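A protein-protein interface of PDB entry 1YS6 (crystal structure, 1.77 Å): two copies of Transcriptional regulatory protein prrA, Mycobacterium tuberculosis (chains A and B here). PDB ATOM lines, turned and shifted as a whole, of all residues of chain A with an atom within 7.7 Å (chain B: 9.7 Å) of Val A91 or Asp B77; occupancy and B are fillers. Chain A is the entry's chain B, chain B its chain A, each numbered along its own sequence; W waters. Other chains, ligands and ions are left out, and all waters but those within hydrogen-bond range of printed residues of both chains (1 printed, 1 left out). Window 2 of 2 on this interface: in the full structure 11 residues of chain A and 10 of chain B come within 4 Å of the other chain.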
ATOM      1  N   ASN A  60      20.578 -10.802 -20.056  1.00  0.00           N
ATOM      2  CA  ASN A  60      21.854 -11.437 -20.422  1.00  0.00           C
ATOM      3  C   ASN A  60      23.024 -10.485 -20.246  1.00  0.00           C
ATOM      4  O   ASN A  60      23.244  -9.567 -21.077  1.00  0.00           O
ATOM      5  CB  ASN A  60      21.741 -11.856 -21.869  1.00  0.00           C
ATOM      6  CG  ASN A  60      20.674 -12.892 -22.082  1.00  0.00           C
ATOM      7  OD1 ASN A  60      20.744 -14.002 -21.535  1.00  0.00           O
ATOM      8  ND2 ASN A  60      19.676 -12.553 -22.890  1.00  0.00           N
ATOM      9  N   SER A  86      14.948  -8.078 -22.625  1.00  0.00           N
ATOM     10  CA  SER A  86      15.673  -9.077 -23.399  1.00  0.00           C
ATOM     11  C   SER A  86      15.600  -8.808 -24.876  1.00  0.00           C
ATOM     12  O   SER A  86      14.658  -8.164 -25.343  1.00  0.00           O
ATOM     13  CB  SER A  86      15.177 -10.481 -23.071  1.00  0.00           C
ATOM     14  OG  SER A  86      13.915 -10.734 -23.661  1.00  0.00           O
ATOM     15  N   ALA A  87      16.589  -9.316 -25.627  1.00  0.00           N
ATOM     16  CA  ALA A  87      16.500  -9.330 -27.086  1.00  0.00           C
ATOM     17  C   ALA A  87      15.281 -10.127 -27.490  1.00  0.00           C
ATOM     18  O   ALA A  87      14.810 -10.962 -26.714  1.00  0.00           O
ATOM     19  CB  ALA A  87      17.775  -9.953 -27.723  1.00  0.00           C
ATOM     20  N   ARG A  88      14.795  -9.904 -28.714  1.00  0.00           N
ATOM     21  CA  ARG A  88      13.583 -10.569 -29.195  1.00  0.00           C
ATOM     22  C   ARG A  88      13.673 -12.086 -29.074  1.00  0.00           C
ATOM     23  O   ARG A  88      12.768 -12.729 -28.532  1.00  0.00           O
ATOM     24  CB  ARG A  88      13.260 -10.173 -30.648  1.00  0.00           C
ATOM     25  N   SER A  89      14.778 -12.638 -29.579  1.00  0.00           N
ATOM     26  CA  SER A  89      14.964 -14.083 -29.749  1.00  0.00           C
ATOM     27  C   SER A  89      15.227 -14.833 -28.419  1.00  0.00           C
ATOM     28  O   SER A  89      14.999 -16.041 -28.316  1.00  0.00           O
ATOM     29  CB  SER A  89      16.094 -14.332 -30.763  1.00  0.00           C
ATOM     30  OG  SER A  89      15.632 -14.263 -32.114  1.00  0.00           O
ATOM     31  N   SER A  90      15.680 -14.104 -27.414  1.00  0.00           N
ATOM     32  CA  SER A  90      16.019 -14.643 -26.093  1.00  0.00           C
ATOM     33  C   SER A  90      14.776 -14.913 -25.181  1.00  0.00           C
ATOM     34  O   SER A  90      14.708 -14.507 -24.009  1.00  0.00           O
ATOM     35  CB  SER A  90      17.050 -13.722 -25.444  1.00  0.00           C
ATOM     36  OG  SER A  90      17.546 -14.244 -24.211  1.00  0.00           O
ATOM     37  N   VAL A  91      13.815 -15.629 -25.753  1.00  0.00           N
ATOM     38  CA  VAL A  91      12.530 -15.965 -25.133  1.00  0.00           C
ATOM     39  C   VAL A  91      12.633 -16.834 -23.881  1.00  0.00           C
ATOM     40  O   VAL A  91      12.143 -16.468 -22.831  1.00  0.00           O
ATOM     41  CB  VAL A  91      11.614 -16.724 -26.119  1.00  0.00           C
ATOM     42  CG1 VAL A  91      10.241 -17.035 -25.477  1.00  0.00           C
ATOM     43  CG2 VAL A  91      11.448 -15.957 -27.424  1.00  0.00           C
ATOM     44  N   ASP A  92      13.212 -18.022 -24.028  1.00  0.00           N
ATOM     45  CA  ASP A  92      13.023 -19.077 -23.050  1.00  0.00           C
ATOM     46  C   ASP A  92      14.163 -18.868 -22.116  1.00  0.00           C
ATOM     47  O   ASP A  92      15.132 -19.636 -22.160  1.00  0.00           O
ATOM     48  CB  ASP A  92      12.985 -20.495 -23.715  1.00  0.00           C
ATOM     49  CG  ASP A  92      14.261 -20.842 -24.475  1.00  0.00           C
ATOM     50  OD1 ASP A  92      14.621 -22.031 -24.515  1.00  0.00           O
ATOM     51  OD2 ASP A  92      14.917 -19.929 -25.036  1.00  0.00           O
ATOM     52  N   ASP A  93      14.017 -17.840 -21.256  1.00  0.00           N
ATOM     53  CA  ASP A  93      15.132 -17.019 -20.833  1.00  0.00           C
ATOM     54  C   ASP A  93      14.666 -15.625 -20.234  1.00  0.00           C
ATOM     55  O   ASP A  93      14.891 -15.334 -19.035  1.00  0.00           O
ATOM     56  CB  ASP A  93      16.110 -16.868 -22.015  1.00  0.00           C
ATOM     57  CG  ASP A  93      17.473 -16.250 -21.612  1.00  0.00           C
ATOM     58  OD1 ASP A  93      18.476 -16.463 -22.329  1.00  0.00           O
ATOM     59  OD2 ASP A  93      17.531 -15.528 -20.600  1.00  0.00           O
ATOM     60  N   ARG A  94      13.986 -14.783 -21.024  1.00  0.00           N
ATOM     61  CA  ARG A  94      13.172 -13.723 -20.384  1.00  0.00           C
ATOM     62  C   ARG A  94      12.081 -14.388 -19.494  1.00  0.00           C
ATOM     63  O   ARG A  94      11.730 -13.886 -18.425  1.00  0.00           O
ATOM     64  CB  ARG A  94      12.514 -12.788 -21.401  1.00  0.00           C
ATOM     65  CG  ARG A  94      11.115 -13.234 -21.821  1.00  0.00           C
ATOM     66  CD  ARG A  94      10.523 -12.334 -22.865  1.00  0.00           C
ATOM     67  NE  ARG A  94      11.487 -12.032 -23.909  1.00  0.00           N
ATOM     68  CZ  ARG A  94      11.423 -12.462 -25.159  1.00  0.00           C
ATOM     69  NH1 ARG A  94      10.425 -13.234 -25.561  1.00  0.00           N
ATOM     70  NH2 ARG A  94      12.379 -12.107 -26.007  1.00  0.00           N
ATOM     71  N   VAL A  95      11.560 -15.519 -19.954  1.00  0.00           N
ATOM     72  CA  VAL A  95      10.603 -16.292 -19.181  1.00  0.00           C
ATOM     73  C   VAL A  95      11.214 -16.704 -17.843  1.00  0.00           C
ATOM     74  O   VAL A  95      10.536 -16.677 -16.802  1.00  0.00           O
ATOM     75  CB  VAL A  95      10.119 -17.509 -20.000  1.00  0.00           C
ATOM     76  CG1 VAL A  95       9.625 -18.650 -19.108  1.00  0.00           C
ATOM     77  CG2 VAL A  95       9.041 -17.065 -20.978  1.00  0.00           C
ATOM     78  N   ALA A  96      12.494 -17.064 -17.869  1.00  0.00           N
ATOM     79  CA  ALA A  96      13.207 -17.391 -16.644  1.00  0.00           C
ATOM     80  C   ALA A  96      13.187 -16.219 -15.630  1.00  0.00           C
ATOM     81  O   ALA A  96      12.978 -16.445 -14.418  1.00  0.00           O
ATOM     82  CB  ALA A  96      14.618 -17.848 -16.961  1.00  0.00           C
ATOM     83  N   GLY A  97      13.326 -14.987 -16.118  1.00  0.00           N
ATOM     84  CA  GLY A  97      13.351 -13.816 -15.219  1.00  0.00           C
ATOM     85  C   GLY A  97      11.986 -13.596 -14.575  1.00  0.00           C
ATOM     86  O   GLY A  97      11.879 -13.250 -13.388  1.00  0.00           O
ATOM     87  N   LEU A  98      10.944 -13.786 -15.370  1.00  0.00           N
ATOM     88  CA  LEU A  98       9.571 -13.654 -14.920  1.00  0.00           C
ATOM     89  C   LEU A  98       9.292 -14.747 -13.909  1.00  0.00           C
ATOM     90  O   LEU A  98       8.797 -14.496 -12.815  1.00  0.00           O
ATOM     91  CB  LEU A  98       8.586 -13.689 -16.074  1.00  0.00           C
ATOM     92  CG  LEU A  98       8.688 -12.543 -17.107  1.00  0.00           C
ATOM     93  CD1 LEU A  98       7.600 -12.684 -18.128  1.00  0.00           C
ATOM     94  CD2 LEU A  98       8.526 -11.205 -16.392  1.00  0.00           C
ATOM     95  N   VAL A 107      10.724  -6.455 -24.548  1.00  0.00           N
ATOM     96  CA  VAL A 107      11.660  -6.945 -25.543  1.00  0.00           C
ATOM     97  C   VAL A 107      12.348  -5.833 -26.333  1.00  0.00           C
ATOM     98  O   VAL A 107      11.715  -4.856 -26.761  1.00  0.00           O
ATOM     99  CB  VAL A 107      10.923  -7.896 -26.483  1.00  0.00           C
ATOM    100  CG1 VAL A 107      11.779  -8.312 -27.691  1.00  0.00           C
ATOM    101  CG2 VAL A 107      10.395  -9.094 -25.684  1.00  0.00           C
ATOM    102  N   ASN A 198       2.293 -10.091 -24.035  1.00  0.00           N
ATOM    103  CA  ASN A 198       1.655 -11.309 -23.560  1.00  0.00           C
ATOM    104  C   ASN A 198       1.908 -11.609 -22.080  1.00  0.00           C
ATOM    105  O   ASN A 198       1.610 -12.709 -21.597  1.00  0.00           O
ATOM    106  CB  ASN A 198       1.965 -12.499 -24.479  1.00  0.00           C
ATOM    107  CG  ASN A 198       3.398 -12.904 -24.450  1.00  0.00           C
ATOM    108  OD1 ASN A 198       4.147 -12.502 -23.569  1.00  0.00           O
ATOM    109  ND2 ASN A 198       3.799 -13.728 -25.403  1.00  0.00           N
ATOM    110  N   VAL A 202       1.444 -15.220 -20.046  1.00  0.00           N
ATOM    111  CA  VAL A 202       2.625 -15.901 -19.537  1.00  0.00           C
ATOM    112  C   VAL A 202       2.369 -16.180 -18.049  1.00  0.00           C
ATOM    113  O   VAL A 202       2.573 -17.281 -17.560  1.00  0.00           O
ATOM    114  CB  VAL A 202       3.848 -14.971 -19.795  1.00  0.00           C
ATOM    115  CG1 VAL A 202       4.997 -15.252 -18.911  1.00  0.00           C
ATOM    116  CG2 VAL A 202       4.278 -15.001 -21.314  1.00  0.00           C
ATOM    117  N   TYR A 206       1.986 -19.703 -15.782  1.00  0.00           N
ATOM    118  CA  TYR A 206       2.699 -20.035 -14.545  1.00  0.00           C
ATOM    119  C   TYR A 206       1.774 -20.347 -13.371  1.00  0.00           C
ATOM    120  O   TYR A 206       1.922 -21.377 -12.721  1.00  0.00           O
ATOM    121  CB  TYR A 206       3.701 -18.937 -14.137  1.00  0.00           C
ATOM    122  CG  TYR A 206       4.717 -18.472 -15.186  1.00  0.00           C
ATOM    123  CD1 TYR A 206       5.370 -19.344 -16.048  1.00  0.00           C
ATOM    124  CD2 TYR A 206       5.012 -17.116 -15.273  1.00  0.00           C
ATOM    125  CE1 TYR A 206       6.309 -18.851 -17.000  1.00  0.00           C
ATOM    126  CE2 TYR A 206       5.891 -16.628 -16.165  1.00  0.00           C
ATOM    127  CZ  TYR A 206       6.542 -17.464 -17.026  1.00  0.00           C
ATOM    128  OH  TYR A 206       7.396 -16.830 -17.897  1.00  0.00           O
ATOM    129  N   ARG B  51       6.710 -28.733 -21.613  1.00  0.00           N
ATOM    130  CA  ARG B  51       8.059 -28.217 -21.320  1.00  0.00           C
ATOM    131  C   ARG B  51       8.982 -29.288 -20.739  1.00  0.00           C
ATOM    132  O   ARG B  51       9.209 -29.417 -19.570  1.00  0.00           O
ATOM    133  CB  ARG B  51       7.982 -26.957 -20.459  1.00  0.00           C
ATOM    134  CG  ARG B  51       7.322 -25.800 -21.202  1.00  0.00           C
ATOM    135  CD  ARG B  51       6.324 -25.068 -20.293  1.00  0.00           C
ATOM    136  NE  ARG B  51       6.252 -23.637 -20.588  1.00  0.00           N
ATOM    137  CZ  ARG B  51       6.887 -22.681 -19.900  1.00  0.00           C
ATOM    138  NH1 ARG B  51       7.661 -22.991 -18.858  1.00  0.00           N
ATOM    139  NH2 ARG B  51       6.752 -21.405 -20.260  1.00  0.00           N
ATOM    140  N   VAL B  69      11.594 -31.070 -36.760  1.00  0.00           N
ATOM    141  CA  VAL B  69      11.334 -30.723 -35.359  1.00  0.00           C
ATOM    142  C   VAL B  69      12.396 -29.834 -34.794  1.00  0.00           C
ATOM    143  O   VAL B  69      12.074 -28.846 -34.130  1.00  0.00           O
ATOM    144  CB  VAL B  69      11.204 -31.979 -34.427  1.00  0.00           C
ATOM    145  CG1 VAL B  69      11.193 -31.514 -32.881  1.00  0.00           C
ATOM    146  CG2 VAL B  69       9.956 -32.717 -34.774  1.00  0.00           C
ATOM    147  N   VAL B  70      13.670 -30.211 -34.953  1.00  0.00           N
ATOM    148  CA  VAL B  70      14.784 -29.402 -34.400  1.00  0.00           C
ATOM    149  C   VAL B  70      14.777 -28.008 -35.000  1.00  0.00           C
ATOM    150  O   VAL B  70      14.896 -27.014 -34.299  1.00  0.00           O
ATOM    151  CB  VAL B  70      16.142 -30.085 -34.713  1.00  0.00           C
ATOM    152  CG1 VAL B  70      17.304 -29.199 -34.313  1.00  0.00           C
ATOM    153  CG2 VAL B  70      16.233 -31.343 -33.892  1.00  0.00           C
ATOM    154  N   THR B  71      14.557 -27.952 -36.322  1.00  0.00           N
ATOM    155  CA  THR B  71      14.479 -26.675 -37.057  1.00  0.00           C
ATOM    156  C   THR B  71      13.353 -25.802 -36.519  1.00  0.00           C
ATOM    157  O   THR B  71      13.556 -24.589 -36.254  1.00  0.00           O
ATOM    158  CB  THR B  71      14.267 -26.942 -38.561  1.00  0.00           C
ATOM    159  OG1 THR B  71      15.390 -27.667 -39.062  1.00  0.00           O
ATOM    160  CG2 THR B  71      14.181 -25.633 -39.354  1.00  0.00           C
ATOM    161  N   ALA B  72      12.188 -26.394 -36.325  1.00  0.00           N
ATOM    162  CA  ALA B  72      11.039 -25.592 -35.834  1.00  0.00           C
ATOM    163  C   ALA B  72      11.369 -25.136 -34.432  1.00  0.00           C
ATOM    164  O   ALA B  72      11.132 -24.012 -34.088  1.00  0.00           O
ATOM    165  CB  ALA B  72       9.755 -26.422 -35.843  1.00  0.00           C
ATOM    166  N   LEU B  73      11.876 -26.045 -33.596  1.00  0.00           N
ATOM    167  CA  LEU B  73      12.197 -25.647 -32.202  1.00  0.00           C
ATOM    168  C   LEU B  73      13.169 -24.497 -32.161  1.00  0.00           C
ATOM    169  O   LEU B  73      12.957 -23.553 -31.448  1.00  0.00           O
ATOM    170  CB  LEU B  73      12.830 -26.791 -31.431  1.00  0.00           C
ATOM    171  CG  LEU B  73      11.888 -27.906 -30.997  1.00  0.00           C
ATOM    172  CD1 LEU B  73      12.708 -28.963 -30.285  1.00  0.00           C
ATOM    173  CD2 LEU B  73      10.820 -27.378 -30.066  1.00  0.00           C
ATOM    174  N   ARG B  74      14.259 -24.591 -32.918  1.00  0.00           N
ATOM    175  CA  ARG B  74      15.247 -23.557 -32.890  1.00  0.00           C
ATOM    176  C   ARG B  74      14.725 -22.250 -33.498  1.00  0.00           C
ATOM    177  O   ARG B  74      15.063 -21.186 -33.016  1.00  0.00           O
ATOM    178  CB  ARG B  74      16.580 -23.951 -33.516  1.00  0.00           C
ATOM    179  CG  ARG B  74      17.285 -25.183 -32.897  1.00  0.00           C
ATOM    180  CD  ARG B  74      17.193 -25.204 -31.337  1.00  0.00           C
ATOM    181  NE  ARG B  74      18.021 -26.281 -30.786  1.00  0.00           N
ATOM    182  CZ  ARG B  74      17.781 -26.970 -29.663  1.00  0.00           C
ATOM    183  NH1 ARG B  74      16.698 -26.725 -28.933  1.00  0.00           N
ATOM    184  NH2 ARG B  74      18.633 -27.950 -29.302  1.00  0.00           N
ATOM    185  N   ALA B  75      13.913 -22.355 -34.531  1.00  0.00           N
ATOM    186  CA  ALA B  75      13.313 -21.193 -35.207  1.00  0.00           C
ATOM    187  C   ALA B  75      12.423 -20.448 -34.225  1.00  0.00           C
ATOM    188  O   ALA B  75      12.324 -19.210 -34.252  1.00  0.00           O
ATOM    189  CB  ALA B  75      12.461 -21.678 -36.371  1.00  0.00           C
ATOM    190  N   MET B  76      11.781 -21.214 -33.356  1.00  0.00           N
ATOM    191  CA  MET B  76      10.945 -20.640 -32.301  1.00  0.00           C
ATOM    192  C   MET B  76      11.662 -20.285 -31.014  1.00  0.00           C
ATOM    193  O   MET B  76      11.009 -20.110 -29.978  1.00  0.00           O
ATOM    194  CB  MET B  76       9.823 -21.624 -31.999  1.00  0.00           C
ATOM    195  CG  MET B  76       8.862 -21.754 -33.149  1.00  0.00           C
ATOM    196  SD  MET B  76       7.511 -22.870 -32.825  1.00  0.00           S
ATOM    197  CE  MET B  76       8.325 -24.415 -32.407  1.00  0.00           C
ATOM    198  N   ASP B  77      12.993 -20.212 -31.063  1.00  0.00           N
ATOM    199  CA  ASP B  77      13.817 -19.804 -29.949  1.00  0.00           C
ATOM    200  C   ASP B  77      13.658 -20.700 -28.735  1.00  0.00           C
ATOM    201  O   ASP B  77      13.801 -20.236 -27.606  1.00  0.00           O
ATOM    202  CB  ASP B  77      13.502 -18.322 -29.564  1.00  0.00           C
ATOM    203  CG  ASP B  77      13.545 -17.401 -30.764  1.00  0.00           C
ATOM    204  OD1 ASP B  77      14.503 -17.597 -31.567  1.00  0.00           O
ATOM    205  OD2 ASP B  77      12.651 -16.493 -30.922  1.00  0.00           O
ATOM    206  N   ASN B  78      13.397 -21.976 -28.973  1.00  0.00           N
ATOM    207  CA  ASN B  78      13.298 -22.920 -27.899  1.00  0.00           C
ATOM    208  C   ASN B  78      14.597 -23.654 -27.782  1.00  0.00           C
ATOM    209  O   ASN B  78      14.908 -24.433 -28.666  1.00  0.00           O
ATOM    210  CB  ASN B  78      12.178 -23.897 -28.145  1.00  0.00           C
ATOM    211  CG  ASN B  78      11.969 -24.843 -26.976  1.00  0.00           C
ATOM    212  OD1 ASN B  78      12.865 -25.026 -26.133  1.00  0.00           O
ATOM    213  ND2 ASN B  78      10.768 -25.410 -26.894  1.00  0.00           N
ATOM    214  N   ASP B  79      15.335 -23.395 -26.709  1.00  0.00           N
ATOM    215  CA  ASP B  79      16.674 -23.956 -26.608  1.00  0.00           C
ATOM    216  C   ASP B  79      16.733 -25.281 -25.870  1.00  0.00           C
ATOM    217  O   ASP B  79      17.786 -25.610 -25.345  1.00  0.00           O
ATOM    218  CB  ASP B  79      17.727 -22.982 -26.071  1.00  0.00           C
ATOM    219  CG  ASP B  79      17.999 -21.829 -27.048  1.00  0.00           C
ATOM    220  OD1 ASP B  79      18.221 -22.101 -28.260  1.00  0.00           O
ATOM    221  OD2 ASP B  79      17.903 -20.676 -26.617  1.00  0.00           O
ATOM    222  N   VAL B  80      15.613 -25.980 -25.803  1.00  0.00           N
ATOM    223  CA  VAL B  80      15.526 -27.265 -25.058  1.00  0.00           C
ATOM    224  C   VAL B  80      16.607 -28.184 -25.574  1.00  0.00           C
ATOM    225  O   VAL B  80      16.797 -28.205 -26.775  1.00  0.00           O
ATOM    226  CB  VAL B  80      14.098 -27.906 -25.162  1.00  0.00           C
ATOM    227  CG1 VAL B  80      13.675 -28.150 -26.579  1.00  0.00           C
ATOM    228  CG2 VAL B  80      13.920 -29.231 -24.354  1.00  0.00           C
ATOM    229  N   ARG B 126      22.041 -27.862 -19.330  1.00  0.00           N
ATOM    230  CA  ARG B 126      20.877 -26.994 -19.152  1.00  0.00           C
ATOM    231  C   ARG B 126      20.737 -26.481 -17.691  1.00  0.00           C
ATOM    232  O   ARG B 126      20.296 -25.342 -17.455  1.00  0.00           O
ATOM    233  CB  ARG B 126      19.600 -27.715 -19.556  1.00  0.00           C
ATOM    234  CG  ARG B 126      18.620 -26.668 -20.106  1.00  0.00           C
ATOM    235  CD  ARG B 126      17.142 -27.060 -20.116  1.00  0.00           C
ATOM    236  NE  ARG B 126      16.400 -26.160 -21.014  1.00  0.00           N
ATOM    237  CZ  ARG B 126      15.078 -26.148 -21.169  1.00  0.00           C
ATOM    238  NH1 ARG B 126      14.298 -26.971 -20.478  1.00  0.00           N
ATOM    239  NH2 ARG B 126      14.537 -25.296 -22.020  1.00  0.00           N
ATOM    240  N   ASP B 159      26.253 -17.328 -38.139  1.00  0.00           N
ATOM    241  CA  ASP B 159      25.035 -17.886 -37.618  1.00  0.00           C
ATOM    242  C   ASP B 159      25.400 -19.233 -37.000  1.00  0.00           C
ATOM    243  O   ASP B 159      25.772 -20.173 -37.702  1.00  0.00           O
ATOM    244  CB  ASP B 159      24.004 -18.010 -38.731  1.00  0.00           C
ATOM    245  CG  ASP B 159      22.701 -18.647 -38.264  1.00  0.00           C
ATOM    246  OD1 ASP B 159      22.337 -18.532 -37.069  1.00  0.00           O
ATOM    247  OD2 ASP B 159      22.043 -19.278 -39.109  1.00  0.00           O
ATOM    248  N   LYS B 162      22.941 -23.262 -31.030  1.00  0.00           N
ATOM    249  CA  LYS B 162      23.176 -23.056 -29.597  1.00  0.00           C
ATOM    250  C   LYS B 162      24.456 -23.792 -29.156  1.00  0.00           C
ATOM    251  O   LYS B 162      25.338 -23.211 -28.523  1.00  0.00           O
ATOM    252  CB  LYS B 162      21.956 -23.541 -28.778  1.00  0.00           C
ATOM    253  CG  LYS B 162      22.198 -23.467 -27.246  1.00  0.00           C
ATOM    254  CD  LYS B 162      21.169 -24.283 -26.491  1.00  0.00           C
ATOM    255  CE  LYS B 162      21.445 -25.797 -26.612  1.00  0.00           C
ATOM    256  NZ  LYS B 162      20.174 -26.492 -26.444  1.00  0.00           N
HETATM  257  O   HOH W   1      12.940 -24.105 -23.642  1.00  0.00           O
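N of Asp B79 is in hydrogen-bond range of OD1 of Asp A92, at 2.7 Å. OD2 of Asp A92 lies close to O of Asp B77, 2.8 Å away.
No position is printed for both chains. Of the 5 pairs that touch across the chains among the printed residues, none has its exchanged pair printed and touching as well.
O of Ser A89 touches CB of Asp B77, at 3.0 Å. OD2 of Asp B77 touches CG2 of Val A91, at 3.7 Å. Asn B78 touches Asp A92.
Of the 18 printed residues of chain A, 3 touch a printed residue of chain B. Hydrophobic or aromatic side chains of chain A within 4 Å of the printed part of chain B: Val A91. Among the printed residues, 5 pairs touch across the chains. Among the printed residues, no Asp or Glu carboxylate lies within 4 Å of a Lys or Arg side-chain nitrogen of the other chain.
Water W1 lies within hydrogen-bond range of the guanidinium group of Arg B126 (2.6 Å), the side-chain amide oxygen of Asn B78 (2.7 Å) and the side-chain carboxylate of Asp A92 (2.8 Å).
O of Leu B73 sits at hydrogen-bond distance from N of Asn B78 (3.0 Å). The guanidinium group (NH1) of Arg B74 is in hydrogen-bond range of the backbone carbonyl oxygen (O) of Asn B78 (2.9 Å). The side-chain amide oxygen (OD1) of Asn B78 sits at hydrogen-bond distance from the backbone NH (N) of Val B80. The backbone carbonyl oxygen (O) of Asp B79 is in hydrogen-bond range of the side-chain amino group (NZ) of Lys B162, at 2.8 Å.
Val A91 touches just one residue of chain B: Asp B77. Of chain A, only Ser A89 (3.0 Å), Val A91 (3.7 Å) and Asp A92 (2.8 Å) come within 4 Å of Asp B77. Asp A92 touches just these residues of chain B: Asp B77, Asn B78 and Asp B79. No residue of chain B comes within 4 Å of Arg A94. Of the printed residues of chain A, Asn B78 touches Asp A92. Printed residues of chain A within 4 Å of Asp B79: Asp A92 (2.7 Å). Leu A98 touches none of the printed residues of chain B. The nearest residue of chain B that does not touch Val A91 is Met B76 (4.9 Å). The nearest printed residue of chain A that does not touch Asp B79 is Ser A89 (5.7 Å).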
